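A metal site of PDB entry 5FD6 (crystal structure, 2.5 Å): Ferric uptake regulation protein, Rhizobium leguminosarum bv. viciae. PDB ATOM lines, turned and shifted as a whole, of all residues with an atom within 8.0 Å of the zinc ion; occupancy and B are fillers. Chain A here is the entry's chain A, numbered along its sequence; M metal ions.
The side-chain carboxylate of Glu 84 is in hydrogen-bond range of a ring nitrogen (NE2) of His 36, 3.3 Å away.
The backbone carbonyl oxygen of Glu 84 is in hydrogen-bond range of the backbone NH of Ala 72 (2.9 Å).
A ring nitrogen (ND1) of His 91 lies close to the side-chain carboxylate of Glu 104.
O of His 36 sits at hydrogen-bond distance from NE of Arg 82 (2.6 Å).
CE1 of His 36 touches the zinc ion, 2.8 Å away.
Within 4 Å of the zinc ion: His 36, Glu 84, His 91 and His 93.
The zinc ion is bound by OE2 of Glu 84 (2.0 Å), NE2 of His 93 (2.1 Å) and NE2 of His 91 (2.2 Å).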
ATOM      1  N   GLU A  34       5.225  -1.942 -17.773  1.00  0.00           N
ATOM      2  CA  GLU A  34       6.307  -1.359 -16.984  1.00  0.00           C
ATOM      3  C   GLU A  34       6.579  -2.134 -15.687  1.00  0.00           C
ATOM      4  O   GLU A  34       7.629  -1.936 -15.076  1.00  0.00           O
ATOM      5  CB  GLU A  34       5.978   0.099 -16.657  1.00  0.00           C
ATOM      6  CG  GLU A  34       6.063   1.007 -17.872  1.00  0.00           C
ATOM      7  CD  GLU A  34       6.099   2.481 -17.535  1.00  0.00           C
ATOM      8  OE1 GLU A  34       6.503   2.841 -16.401  1.00  0.00           O
ATOM      9  OE2 GLU A  34       5.739   3.286 -18.420  1.00  0.00           O
ATOM     10  N   ASP A  35       5.621  -2.934 -15.229  1.00  0.00           N
ATOM     11  CA  ASP A  35       5.868  -3.972 -14.260  1.00  0.00           C
ATOM     12  C   ASP A  35       6.479  -5.057 -15.120  1.00  0.00           C
ATOM     13  O   ASP A  35       6.033  -5.255 -16.231  1.00  0.00           O
ATOM     14  CB  ASP A  35       4.555  -4.409 -13.541  1.00  0.00           C
ATOM     15  CG  ASP A  35       3.671  -5.299 -14.417  1.00  0.00           C
ATOM     16  OD1 ASP A  35       3.364  -4.900 -15.554  1.00  0.00           O
ATOM     17  OD2 ASP A  35       3.273  -6.395 -13.985  1.00  0.00           O
ATOM     18  N   HIS A  36       7.541  -5.698 -14.667  1.00  0.00           N
ATOM     19  CA  HIS A  36       8.348  -6.528 -15.567  1.00  0.00           C
ATOM     20  C   HIS A  36       7.780  -7.947 -15.497  1.00  0.00           C
ATOM     21  O   HIS A  36       8.255  -8.759 -14.709  1.00  0.00           O
ATOM     22  CB  HIS A  36       9.831  -6.487 -15.171  1.00  0.00           C
ATOM     23  CG  HIS A  36      10.429  -5.107 -15.208  1.00  0.00           C
ATOM     24  ND1 HIS A  36      11.104  -4.570 -14.142  1.00  0.00           N
ATOM     25  CD2 HIS A  36      10.421  -4.154 -16.160  1.00  0.00           C
ATOM     26  CE1 HIS A  36      11.507  -3.350 -14.446  1.00  0.00           C
ATOM     27  NE2 HIS A  36      11.111  -3.078 -15.670  1.00  0.00           N
ATOM     28  N   ALA A  72      15.361  -8.355 -21.808  1.00  0.00           N
ATOM     29  CA  ALA A  72      16.249  -8.584 -20.683  1.00  0.00           C
ATOM     30  C   ALA A  72      15.505  -9.417 -19.612  1.00  0.00           C
ATOM     31  O   ALA A  72      14.458  -9.017 -19.137  1.00  0.00           O
ATOM     32  CB  ALA A  72      16.660  -7.250 -20.084  1.00  0.00           C
ATOM     33  N   HIS A  74      15.462 -10.851 -15.772  1.00  0.00           N
ATOM     34  CA  HIS A  74      15.963 -10.511 -14.437  1.00  0.00           C
ATOM     35  C   HIS A  74      15.510 -11.536 -13.416  1.00  0.00           C
ATOM     36  O   HIS A  74      14.318 -11.761 -13.259  1.00  0.00           O
ATOM     37  CB  HIS A  74      15.477  -9.133 -14.016  1.00  0.00           C
ATOM     38  CG  HIS A  74      16.251  -8.016 -14.640  1.00  0.00           C
ATOM     39  ND1 HIS A  74      17.489  -7.628 -14.172  1.00  0.00           N
ATOM     40  CD2 HIS A  74      15.962  -7.218 -15.690  1.00  0.00           C
ATOM     41  CE1 HIS A  74      17.931  -6.634 -14.925  1.00  0.00           C
ATOM     42  NE2 HIS A  74      17.032  -6.380 -15.848  1.00  0.00           N
ATOM     43  N   PHE A  76      15.347 -11.666  -9.808  1.00  0.00           N
ATOM     44  CA  PHE A  76      15.344 -11.066  -8.497  1.00  0.00           C
ATOM     45  C   PHE A  76      15.015 -12.153  -7.478  1.00  0.00           C
ATOM     46  O   PHE A  76      14.344 -13.140  -7.812  1.00  0.00           O
ATOM     47  CB  PHE A  76      14.331  -9.925  -8.496  1.00  0.00           C
ATOM     48  CG  PHE A  76      14.658  -8.827  -9.488  1.00  0.00           C
ATOM     49  CD1 PHE A  76      15.849  -8.105  -9.379  1.00  0.00           C
ATOM     50  CD2 PHE A  76      13.790  -8.499 -10.520  1.00  0.00           C
ATOM     51  CE1 PHE A  76      16.145  -7.093 -10.267  1.00  0.00           C
ATOM     52  CE2 PHE A  76      14.091  -7.493 -11.412  1.00  0.00           C
ATOM     53  CZ  PHE A  76      15.270  -6.789 -11.297  1.00  0.00           C
ATOM     54  N   ARG A  82      11.752 -12.062 -14.129  1.00  0.00           N
ATOM     55  CA  ARG A  82      11.050 -10.897 -14.636  1.00  0.00           C
ATOM     56  C   ARG A  82      11.667 -10.481 -15.953  1.00  0.00           C
ATOM     57  O   ARG A  82      12.878 -10.530 -16.119  1.00  0.00           O
ATOM     58  CB  ARG A  82      11.188  -9.726 -13.663  1.00  0.00           C
ATOM     59  CG  ARG A  82      10.946 -10.025 -12.186  1.00  0.00           C
ATOM     60  CD  ARG A  82       9.541 -10.475 -11.873  1.00  0.00           C
ATOM     61  NE  ARG A  82       8.534  -9.466 -12.206  1.00  0.00           N
ATOM     62  CZ  ARG A  82       7.245  -9.550 -11.889  1.00  0.00           C
ATOM     63  NH1 ARG A  82       6.804 -10.593 -11.224  1.00  0.00           N
ATOM     64  NH2 ARG A  82       6.378  -8.602 -12.248  1.00  0.00           N
ATOM     65  N   TYR A  83      10.820 -10.059 -16.884  1.00  0.00           N
ATOM     66  CA  TYR A  83      11.251  -9.765 -18.230  1.00  0.00           C
ATOM     67  C   TYR A  83      10.830  -8.372 -18.630  1.00  0.00           C
ATOM     68  O   TYR A  83       9.752  -7.907 -18.253  1.00  0.00           O
ATOM     69  CB  TYR A  83      10.659 -10.785 -19.176  1.00  0.00           C
ATOM     70  CG  TYR A  83      11.180 -12.191 -19.005  1.00  0.00           C
ATOM     71  CD1 TYR A  83      12.264 -12.650 -19.737  1.00  0.00           C
ATOM     72  CD2 TYR A  83      10.563 -13.073 -18.119  1.00  0.00           C
ATOM     73  CE1 TYR A  83      12.733 -13.948 -19.597  1.00  0.00           C
ATOM     74  CE2 TYR A  83      11.024 -14.378 -17.980  1.00  0.00           C
ATOM     75  CZ  TYR A  83      12.107 -14.808 -18.710  1.00  0.00           C
ATOM     76  OH  TYR A  83      12.574 -16.088 -18.574  1.00  0.00           O
ATOM     77  N   GLU A  84      11.672  -7.706 -19.417  1.00  0.00           N
ATOM     78  CA  GLU A  84      11.305  -6.420 -19.998  1.00  0.00           C
ATOM     79  C   GLU A  84      11.942  -6.187 -21.341  1.00  0.00           C
ATOM     80  O   GLU A  84      12.943  -6.825 -21.694  1.00  0.00           O
ATOM     81  CB  GLU A  84      11.712  -5.285 -19.059  1.00  0.00           C
ATOM     82  CG  GLU A  84      13.211  -5.192 -18.812  1.00  0.00           C
ATOM     83  CD  GLU A  84      13.613  -3.969 -18.013  1.00  0.00           C
ATOM     84  OE1 GLU A  84      13.103  -2.858 -18.288  1.00  0.00           O
ATOM     85  OE2 GLU A  84      14.478  -4.110 -17.101  1.00  0.00           O
ATOM     86  N   THR A  85      11.376  -5.226 -22.067  1.00  0.00           N
ATOM     87  CA  THR A  85      11.942  -4.765 -23.319  1.00  0.00           C
ATOM     88  C   THR A  85      13.230  -4.092 -22.920  1.00  0.00           C
ATOM     89  O   THR A  85      13.249  -3.378 -21.911  1.00  0.00           O
ATOM     90  CB  THR A  85      11.048  -3.752 -24.077  1.00  0.00           C
ATOM     91  OG1 THR A  85      10.926  -2.511 -23.346  1.00  0.00           O
ATOM     92  CG2 THR A  85       9.681  -4.347 -24.336  1.00  0.00           C
ATOM     93  N   VAL A  86      14.308  -4.351 -23.654  1.00  0.00           N
ATOM     94  CA  VAL A  86      15.606  -3.749 -23.344  1.00  0.00           C
ATOM     95  C   VAL A  86      15.432  -2.239 -23.097  1.00  0.00           C
ATOM     96  O   VAL A  86      14.895  -1.545 -23.943  1.00  0.00           O
ATOM     97  CB  VAL A  86      16.699  -4.048 -24.399  1.00  0.00           C
ATOM     98  CG1 VAL A  86      16.255  -3.735 -25.828  1.00  0.00           C
ATOM     99  CG2 VAL A  86      17.990  -3.307 -24.072  1.00  0.00           C
ATOM    100  N   PRO A  87      15.841  -1.745 -21.897  1.00  0.00           N
ATOM    101  CA  PRO A  87      15.596  -0.346 -21.591  1.00  0.00           C
ATOM    102  C   PRO A  87      16.556   0.573 -22.344  1.00  0.00           C
ATOM    103  O   PRO A  87      17.765   0.303 -22.414  1.00  0.00           O
ATOM    104  CB  PRO A  87      15.796  -0.255 -20.078  1.00  0.00           C
ATOM    105  CG  PRO A  87      16.501  -1.499 -19.660  1.00  0.00           C
ATOM    106  CD  PRO A  87      16.583  -2.433 -20.820  1.00  0.00           C
ATOM    107  N   GLU A  89      17.363   3.577 -21.556  1.00  0.00           N
ATOM    108  CA  GLU A  89      18.272   4.107 -20.549  1.00  0.00           C
ATOM    109  C   GLU A  89      18.276   3.219 -19.325  1.00  0.00           C
ATOM    110  O   GLU A  89      17.270   2.621 -18.959  1.00  0.00           O
ATOM    111  CB  GLU A  89      17.936   5.548 -20.160  1.00  0.00           C
ATOM    112  CG  GLU A  89      16.495   5.777 -19.741  1.00  0.00           C
ATOM    113  CD  GLU A  89      16.237   7.189 -19.238  1.00  0.00           C
ATOM    114  OE1 GLU A  89      17.041   8.101 -19.533  1.00  0.00           O
ATOM    115  OE2 GLU A  89      15.223   7.384 -18.546  1.00  0.00           O
ATOM    116  N   HIS A  90      19.435   3.161 -18.704  1.00  0.00           N
ATOM    117  CA  HIS A  90      19.627   2.439 -17.466  1.00  0.00           C
ATOM    118  C   HIS A  90      18.669   2.927 -16.374  1.00  0.00           C
ATOM    119  O   HIS A  90      18.368   4.106 -16.270  1.00  0.00           O
ATOM    120  CB  HIS A  90      21.084   2.620 -17.015  1.00  0.00           C
ATOM    121  CG  HIS A  90      21.250   2.558 -15.535  1.00  0.00           C
ATOM    122  ND1 HIS A  90      21.409   1.377 -14.838  1.00  0.00           N
ATOM    123  CD2 HIS A  90      21.245   3.549 -14.604  1.00  0.00           C
ATOM    124  CE1 HIS A  90      21.517   1.649 -13.549  1.00  0.00           C
ATOM    125  NE2 HIS A  90      21.422   2.951 -13.387  1.00  0.00           N
ATOM    126  N   HIS A  91      18.219   1.976 -15.556  1.00  0.00           N
ATOM    127  CA  HIS A  91      17.495   2.259 -14.319  1.00  0.00           C
ATOM    128  C   HIS A  91      17.727   1.112 -13.325  1.00  0.00           C
ATOM    129  O   HIS A  91      18.136   0.009 -13.711  1.00  0.00           O
ATOM    130  CB  HIS A  91      15.993   2.410 -14.585  1.00  0.00           C
ATOM    131  CG  HIS A  91      15.347   1.156 -15.094  1.00  0.00           C
ATOM    132  ND1 HIS A  91      14.867   1.036 -16.374  1.00  0.00           N
ATOM    133  CD2 HIS A  91      15.166  -0.052 -14.516  1.00  0.00           C
ATOM    134  CE1 HIS A  91      14.388  -0.171 -16.559  1.00  0.00           C
ATOM    135  NE2 HIS A  91      14.551  -0.857 -15.443  1.00  0.00           N
ATOM    136  N   ASP A  92      17.414   1.375 -12.071  1.00  0.00           N
ATOM    137  CA  ASP A  92      17.486   0.363 -11.005  1.00  0.00           C
ATOM    138  C   ASP A  92      16.106  -0.190 -10.686  1.00  0.00           C
ATOM    139  O   ASP A  92      15.109   0.239 -11.289  1.00  0.00           O
ATOM    140  CB  ASP A  92      18.203   0.979  -9.782  1.00  0.00           C
ATOM    141  CG  ASP A  92      19.636   1.339 -10.106  1.00  0.00           C
ATOM    142  OD1 ASP A  92      20.267   0.518 -10.793  1.00  0.00           O
ATOM    143  OD2 ASP A  92      20.137   2.420  -9.746  1.00  0.00           O
ATOM    144  N   HIS A  93      16.047  -1.151  -9.777  1.00  0.00           N
ATOM    145  CA  HIS A  93      14.813  -1.887  -9.504  1.00  0.00           C
ATOM    146  C   HIS A  93      14.417  -1.940  -8.042  1.00  0.00           C
ATOM    147  O   HIS A  93      15.264  -2.146  -7.153  1.00  0.00           O
ATOM    148  CB  HIS A  93      14.993  -3.303 -10.001  1.00  0.00           C
ATOM    149  CG  HIS A  93      15.089  -3.409 -11.492  1.00  0.00           C
ATOM    150  ND1 HIS A  93      16.287  -3.437 -12.157  1.00  0.00           N
ATOM    151  CD2 HIS A  93      14.128  -3.488 -12.430  1.00  0.00           C
ATOM    152  CE1 HIS A  93      16.064  -3.552 -13.454  1.00  0.00           C
ATOM    153  NE2 HIS A  93      14.765  -3.589 -13.647  1.00  0.00           N
ATOM    154  N   LEU A  94      13.131  -1.716  -7.806  1.00  0.00           N
ATOM    155  CA  LEU A  94      12.464  -1.936  -6.528  1.00  0.00           C
ATOM    156  C   LEU A  94      11.397  -3.026  -6.767  1.00  0.00           C
ATOM    157  O   LEU A  94      10.661  -2.958  -7.751  1.00  0.00           O
ATOM    158  CB  LEU A  94      11.794  -0.645  -6.089  1.00  0.00           C
ATOM    159  CG  LEU A  94      10.853  -0.584  -4.871  1.00  0.00           C
ATOM    160  CD1 LEU A  94      11.579  -0.900  -3.577  1.00  0.00           C
ATOM    161  CD2 LEU A  94      10.246   0.805  -4.816  1.00  0.00           C
ATOM    162  N   VAL A 102       7.400  -5.399 -10.160  1.00  0.00           N
ATOM    163  CA  VAL A 102       8.618  -4.572 -10.146  1.00  0.00           C
ATOM    164  C   VAL A 102       8.392  -3.111 -10.542  1.00  0.00           C
ATOM    165  O   VAL A 102       7.669  -2.806 -11.508  1.00  0.00           O
ATOM    166  CB  VAL A 102       9.689  -5.182 -11.072  1.00  0.00           C
ATOM    167  CG1 VAL A 102      10.991  -4.385 -10.980  1.00  0.00           C
ATOM    168  CG2 VAL A 102       9.974  -6.632 -10.675  1.00  0.00           C
ATOM    169  N   ILE A 103       9.044  -2.230  -9.792  1.00  0.00           N
ATOM    170  CA  ILE A 103       9.045  -0.805 -10.024  1.00  0.00           C
ATOM    171  C   ILE A 103      10.474  -0.373 -10.394  1.00  0.00           C
ATOM    172  O   ILE A 103      11.411  -0.653  -9.658  1.00  0.00           O
ATOM    173  CB  ILE A 103       8.566  -0.052  -8.746  1.00  0.00           C
ATOM    174  CG1 ILE A 103       7.088  -0.369  -8.482  1.00  0.00           C
ATOM    175  CG2 ILE A 103       8.825   1.459  -8.858  1.00  0.00           C
ATOM    176  CD1 ILE A 103       6.845  -1.659  -7.712  1.00  0.00           C
ATOM    177  N   GLU A 104      10.601   0.298 -11.541  1.00  0.00           N
ATOM    178  CA  GLU A 104      11.868   0.908 -11.998  1.00  0.00           C
ATOM    179  C   GLU A 104      12.072   2.307 -11.411  1.00  0.00           C
ATOM    180  O   GLU A 104      11.117   3.008 -11.109  1.00  0.00           O
ATOM    181  CB  GLU A 104      11.949   0.932 -13.542  1.00  0.00           C
ATOM    182  CG  GLU A 104      10.802   1.595 -14.299  1.00  0.00           C
ATOM    183  CD  GLU A 104      10.677   1.098 -15.746  1.00  0.00           C
ATOM    184  OE1 GLU A 104      11.532   1.472 -16.571  1.00  0.00           O
ATOM    185  OE2 GLU A 104       9.731   0.350 -16.058  1.00  0.00           O
ATOM    186  N   PHE A 105      13.339   2.694 -11.228  1.00  0.00           N
ATOM    187  CA  PHE A 105      13.693   4.021 -10.752  1.00  0.00           C
ATOM    188  C   PHE A 105      15.106   4.419 -11.166  1.00  0.00           C
ATOM    189  O   PHE A 105      15.984   3.569 -11.313  1.00  0.00           O
ATOM    190  CB  PHE A 105      13.502   4.167  -9.232  1.00  0.00           C
ATOM    191  CG  PHE A 105      14.455   3.344  -8.386  1.00  0.00           C
ATOM    192  CD1 PHE A 105      15.682   3.859  -7.983  1.00  0.00           C
ATOM    193  CD2 PHE A 105      14.092   2.074  -7.946  1.00  0.00           C
ATOM    194  CE1 PHE A 105      16.544   3.114  -7.182  1.00  0.00           C
ATOM    195  CE2 PHE A 105      14.951   1.332  -7.153  1.00  0.00           C
ATOM    196  CZ  PHE A 105      16.162   1.851  -6.757  1.00  0.00           C
HETATM  197 ZN    ZN M   1      14.055  -2.970 -15.539  1.00  0.00          ZN
